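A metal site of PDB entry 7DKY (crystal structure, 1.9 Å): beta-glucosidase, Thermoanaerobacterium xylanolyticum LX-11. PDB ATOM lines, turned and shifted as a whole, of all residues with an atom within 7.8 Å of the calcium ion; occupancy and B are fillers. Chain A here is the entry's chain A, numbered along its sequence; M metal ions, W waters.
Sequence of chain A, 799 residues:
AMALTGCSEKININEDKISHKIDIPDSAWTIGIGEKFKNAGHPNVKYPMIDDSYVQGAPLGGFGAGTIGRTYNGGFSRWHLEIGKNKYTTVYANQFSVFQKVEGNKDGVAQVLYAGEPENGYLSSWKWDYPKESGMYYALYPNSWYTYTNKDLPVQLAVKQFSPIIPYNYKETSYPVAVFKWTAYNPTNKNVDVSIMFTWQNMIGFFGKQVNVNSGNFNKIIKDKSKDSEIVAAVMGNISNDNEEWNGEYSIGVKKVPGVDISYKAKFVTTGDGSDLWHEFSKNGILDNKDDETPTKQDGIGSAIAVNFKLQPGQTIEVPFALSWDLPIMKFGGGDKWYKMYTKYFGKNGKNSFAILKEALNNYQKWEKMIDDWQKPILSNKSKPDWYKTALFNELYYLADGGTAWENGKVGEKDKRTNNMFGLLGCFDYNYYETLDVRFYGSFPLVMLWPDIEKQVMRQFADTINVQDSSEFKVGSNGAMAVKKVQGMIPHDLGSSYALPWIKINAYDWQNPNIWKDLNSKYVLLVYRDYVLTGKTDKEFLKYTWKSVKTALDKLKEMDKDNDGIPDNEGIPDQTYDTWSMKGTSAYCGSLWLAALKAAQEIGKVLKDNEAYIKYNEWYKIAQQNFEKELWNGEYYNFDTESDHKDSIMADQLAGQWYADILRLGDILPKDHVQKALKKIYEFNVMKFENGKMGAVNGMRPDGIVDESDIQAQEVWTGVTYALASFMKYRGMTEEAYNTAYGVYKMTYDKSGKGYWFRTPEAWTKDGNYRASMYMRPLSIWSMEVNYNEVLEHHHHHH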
ATOM      1  N   LYS A 557      18.718 -23.684   4.072  1.00  0.00           N
ATOM      2  CA  LYS A 557      19.969 -22.946   4.316  1.00  0.00           C
ATOM      3  C   LYS A 557      20.159 -22.562   5.801  1.00  0.00           C
ATOM      4  O   LYS A 557      21.272 -22.644   6.324  1.00  0.00           O
ATOM      5  CB  LYS A 557      20.009 -21.702   3.431  1.00  0.00           C
ATOM      6  CG  LYS A 557      21.277 -20.862   3.461  1.00  0.00           C
ATOM      7  CD  LYS A 557      22.513 -21.676   3.148  1.00  0.00           C
ATOM      8  CE  LYS A 557      23.611 -20.856   2.506  1.00  0.00           C
ATOM      9  NZ  LYS A 557      24.059 -19.745   3.378  1.00  0.00           N
ATOM     10  N   MET A 559      19.453 -24.304   8.279  1.00  0.00           N
ATOM     11  CA  MET A 559      19.949 -25.479   8.995  1.00  0.00           C
ATOM     12  C   MET A 559      21.453 -25.714   8.877  1.00  0.00           C
ATOM     13  O   MET A 559      21.971 -26.664   9.454  1.00  0.00           O
ATOM     14  CB  MET A 559      19.170 -26.724   8.555  1.00  0.00           C
ATOM     15  CG  MET A 559      17.744 -26.708   9.064  1.00  0.00           C
ATOM     16  SD  MET A 559      16.695 -27.932   8.265  1.00  0.00           S
ATOM     17  CE  MET A 559      15.225 -27.733   9.260  1.00  0.00           C
ATOM     18  N   ASP A 560      22.162 -24.876   8.123  1.00  0.00           N
ATOM     19  CA  ASP A 560      23.638 -24.866   8.134  1.00  0.00           C
ATOM     20  C   ASP A 560      24.118 -24.265   9.466  1.00  0.00           C
ATOM     21  O   ASP A 560      23.948 -23.080   9.678  1.00  0.00           O
ATOM     22  CB  ASP A 560      24.137 -24.015   6.958  1.00  0.00           C
ATOM     23  CG  ASP A 560      25.662 -23.891   6.904  1.00  0.00           C
ATOM     24  OD1 ASP A 560      26.385 -24.714   7.496  1.00  0.00           O
ATOM     25  OD2 ASP A 560      26.138 -22.974   6.226  1.00  0.00           O
ATOM     26  N   LYS A 561      24.693 -25.094  10.327  1.00  0.00           N
ATOM     27  CA  LYS A 561      25.132 -24.688  11.679  1.00  0.00           C
ATOM     28  C   LYS A 561      26.533 -24.064  11.743  1.00  0.00           C
ATOM     29  O   LYS A 561      26.798 -23.251  12.633  1.00  0.00           O
ATOM     30  CB  LYS A 561      25.153 -25.914  12.627  1.00  0.00           C
ATOM     31  CG  LYS A 561      23.838 -26.637  12.830  1.00  0.00           C
ATOM     32  CD  LYS A 561      22.779 -25.764  13.509  1.00  0.00           C
ATOM     33  CE  LYS A 561      21.873 -25.049  12.500  1.00  0.00           C
ATOM     34  NZ  LYS A 561      21.489 -23.684  12.938  1.00  0.00           N
ATOM     35  N   ASP A 562      27.439 -24.452  10.848  1.00  0.00           N
ATOM     36  CA  ASP A 562      28.847 -24.049  10.951  1.00  0.00           C
ATOM     37  C   ASP A 562      29.309 -23.188   9.780  1.00  0.00           C
ATOM     38  O   ASP A 562      30.508 -23.080   9.542  1.00  0.00           O
ATOM     39  CB  ASP A 562      29.731 -25.297  11.093  1.00  0.00           C
ATOM     40  CG  ASP A 562      29.707 -26.173   9.839  1.00  0.00           C
ATOM     41  OD1 ASP A 562      28.796 -25.971   9.003  1.00  0.00           O
ATOM     42  OD2 ASP A 562      30.575 -27.051   9.685  1.00  0.00           O
ATOM     43  N   ASN A 563      28.369 -22.578   9.064  1.00  0.00           N
ATOM     44  CA  ASN A 563      28.662 -21.706   7.924  1.00  0.00           C
ATOM     45  C   ASN A 563      29.546 -22.290   6.770  1.00  0.00           C
ATOM     46  O   ASN A 563      30.274 -21.546   6.101  1.00  0.00           O
ATOM     47  CB  ASN A 563      29.253 -20.376   8.432  1.00  0.00           C
ATOM     48  CG  ASN A 563      28.993 -19.207   7.480  1.00  0.00           C
ATOM     49  OD1 ASN A 563      27.958 -19.144   6.811  1.00  0.00           O
ATOM     50  ND2 ASN A 563      29.930 -18.273   7.431  1.00  0.00           N
ATOM     51  N   ASP A 564      29.490 -23.602   6.521  1.00  0.00           N
ATOM     52  CA  ASP A 564      30.159 -24.178   5.340  1.00  0.00           C
ATOM     53  C   ASP A 564      29.261 -24.157   4.081  1.00  0.00           C
ATOM     54  O   ASP A 564      29.659 -24.696   3.031  1.00  0.00           O
ATOM     55  CB  ASP A 564      30.674 -25.609   5.629  1.00  0.00           C
ATOM     56  CG  ASP A 564      29.544 -26.657   5.632  1.00  0.00           C
ATOM     57  OD1 ASP A 564      28.363 -26.264   5.749  1.00  0.00           O
ATOM     58  OD2 ASP A 564      29.830 -27.866   5.583  1.00  0.00           O
ATOM     59  N   GLY A 565      28.063 -23.556   4.188  1.00  0.00           N
ATOM     60  CA  GLY A 565      27.141 -23.396   3.073  1.00  0.00           C
ATOM     61  C   GLY A 565      26.192 -24.573   2.827  1.00  0.00           C
ATOM     62  O   GLY A 565      25.468 -24.585   1.840  1.00  0.00           O
ATOM     63  N   ILE A 566      26.201 -25.562   3.733  1.00  0.00           N
ATOM     64  CA  ILE A 566      25.498 -26.844   3.537  1.00  0.00           C
ATOM     65  C   ILE A 566      24.692 -27.145   4.819  1.00  0.00           C
ATOM     66  O   ILE A 566      25.239 -27.035   5.924  1.00  0.00           O
ATOM     67  CB  ILE A 566      26.506 -27.994   3.289  1.00  0.00           C
ATOM     68  CG1 ILE A 566      27.427 -27.692   2.088  1.00  0.00           C
ATOM     69  CG2 ILE A 566      25.780 -29.335   3.065  1.00  0.00           C
ATOM     70  CD1 ILE A 566      28.584 -28.636   1.950  1.00  0.00           C
ATOM     71  N   PRO A 567      23.414 -27.570   4.687  1.00  0.00           N
ATOM     72  CA  PRO A 567      22.711 -27.989   5.903  1.00  0.00           C
ATOM     73  C   PRO A 567      23.415 -29.105   6.686  1.00  0.00           C
ATOM     74  O   PRO A 567      24.049 -29.961   6.081  1.00  0.00           O
ATOM     75  CB  PRO A 567      21.336 -28.453   5.388  1.00  0.00           C
ATOM     76  CG  PRO A 567      21.521 -28.684   3.924  1.00  0.00           C
ATOM     77  CD  PRO A 567      22.550 -27.689   3.498  1.00  0.00           C
ATOM     78  N   ASP A 568      23.355 -29.048   8.020  1.00  0.00           N
ATOM     79  CA  ASP A 568      23.985 -30.049   8.900  1.00  0.00           C
ATOM     80  C   ASP A 568      22.968 -31.122   9.316  1.00  0.00           C
ATOM     81  O   ASP A 568      21.934 -30.812   9.920  1.00  0.00           O
ATOM     82  CB  ASP A 568      24.519 -29.403  10.191  1.00  0.00           C
ATOM     83  CG  ASP A 568      25.793 -28.599   9.969  1.00  0.00           C
ATOM     84  OD1 ASP A 568      25.734 -27.520   9.341  1.00  0.00           O
ATOM     85  OD2 ASP A 568      26.864 -29.063  10.425  1.00  0.00           O
ATOM     86  N   ASN A 569      23.291 -32.393   9.049  1.00  0.00           N
ATOM     87  CA  ASN A 569      22.565 -33.501   9.634  1.00  0.00           C
ATOM     88  C   ASN A 569      22.871 -33.473  11.159  1.00  0.00           C
ATOM     89  O   ASN A 569      23.998 -33.155  11.582  1.00  0.00           O
ATOM     90  CB  ASN A 569      22.950 -34.835   8.984  1.00  0.00           C
ATOM     91  CG  ASN A 569      22.545 -34.926   7.502  1.00  0.00           C
ATOM     92  OD1 ASN A 569      23.336 -34.636   6.607  1.00  0.00           O
ATOM     93  ND2 ASN A 569      21.319 -35.339   7.254  1.00  0.00           N
ATOM     94  N   GLY A 584      26.625 -33.867  10.423  1.00  0.00           N
ATOM     95  CA  GLY A 584      27.481 -32.919   9.749  1.00  0.00           C
ATOM     96  C   GLY A 584      27.087 -32.799   8.315  1.00  0.00           C
ATOM     97  O   GLY A 584      25.883 -32.766   7.990  1.00  0.00           O
ATOM     98  N   THR A 585      28.079 -32.769   7.426  1.00  0.00           N
ATOM     99  CA  THR A 585      27.806 -32.781   5.985  1.00  0.00           C
ATOM    100  C   THR A 585      27.741 -34.238   5.564  1.00  0.00           C
ATOM    101  O   THR A 585      28.702 -34.960   5.783  1.00  0.00           O
ATOM    102  CB  THR A 585      28.880 -31.998   5.219  1.00  0.00           C
ATOM    103  OG1 THR A 585      28.819 -30.623   5.606  1.00  0.00           O
ATOM    104  CG2 THR A 585      28.649 -32.092   3.705  1.00  0.00           C
ATOM    105  N   GLU A 630      35.463 -31.544   2.182  1.00  0.00           N
ATOM    106  CA  GLU A 630      35.060 -32.299   3.367  1.00  0.00           C
ATOM    107  C   GLU A 630      34.937 -33.791   3.135  1.00  0.00           C
ATOM    108  O   GLU A 630      35.201 -34.568   4.046  1.00  0.00           O
ATOM    109  CB  GLU A 630      33.736 -31.766   3.903  1.00  0.00           C
ATOM    110  CG  GLU A 630      33.828 -30.387   4.565  1.00  0.00           C
ATOM    111  CD  GLU A 630      32.479 -29.714   4.709  1.00  0.00           C
ATOM    112  OE1 GLU A 630      31.444 -30.429   4.645  1.00  0.00           O
ATOM    113  OE2 GLU A 630      32.449 -28.470   4.858  1.00  0.00           O
ATOM    114  N   THR A 641      30.644 -36.204   7.671  1.00  0.00           N
ATOM    115  CA  THR A 641      31.828 -35.620   8.321  1.00  0.00           C
ATOM    116  C   THR A 641      31.995 -35.936   9.814  1.00  0.00           C
ATOM    117  O   THR A 641      33.080 -35.754  10.341  1.00  0.00           O
ATOM    118  CB  THR A 641      31.866 -34.096   8.132  1.00  0.00           C
ATOM    119  OG1 THR A 641      30.649 -33.528   8.623  1.00  0.00           O
ATOM    120  CG2 THR A 641      32.049 -33.728   6.661  1.00  0.00           C
ATOM    121  N   GLU A 642      30.935 -36.384  10.511  1.00  0.00           N
ATOM    122  CA  GLU A 642      30.975 -36.497  11.986  1.00  0.00           C
ATOM    123  C   GLU A 642      30.514 -37.810  12.664  1.00  0.00           C
ATOM    124  O   GLU A 642      30.703 -37.944  13.860  1.00  0.00           O
ATOM    125  CB  GLU A 642      30.210 -35.328  12.601  1.00  0.00           C
ATOM    126  CG  GLU A 642      30.790 -33.959  12.268  1.00  0.00           C
ATOM    127  CD  GLU A 642      29.982 -32.814  12.857  1.00  0.00           C
ATOM    128  OE1 GLU A 642      29.421 -32.981  13.954  1.00  0.00           O
ATOM    129  OE2 GLU A 642      29.911 -31.740  12.222  1.00  0.00           O
HETATM  130 CA    CA M   1      27.022 -26.951   7.553  1.00  0.00          CA
HETATM  131  O   HOH W   1      26.875 -29.405   6.758  1.00  0.00           O
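N of Lys 561 sits close to OD1 of Asp 568, at 2.8 Å. OD2 of Asp 560 lies within hydrogen-bond range of N of Gly 565, at 2.9 Å. The backbone NH (N) of Asp 568 sits at hydrogen-bond distance from the backbone carbonyl oxygen (O) of Met 559 (3.1 Å). The backbone NH (N) of Asn 563 lies close to the side-chain carboxylate (OD1) of Asp 560 (3.3 Å). The side-chain hydroxyl of Thr 585 sits at hydrogen-bond distance from the side-chain carboxylate of Asp 564 (2.9 Å).
OD1 of Asp 568 binds the calcium ion (2.3 Å). OD1 of Asp 560 is bound to the calcium ion (2.3 Å). The calcium ion is bound by OD1 of Asp 564 (2.4 Å). O of Ile 566 is bound to the calcium ion, 2.4 Å away. The side-chain carboxylate (OD1) of Asp 562 binds the calcium ion (2.5 Å). Water W1 binds the calcium ion.
Water W1 lies within hydrogen-bond range of the side-chain hydroxyl of Thr 585 (2.6 Å) and the backbone carbonyl oxygen of Pro 567 (3.0 Å).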
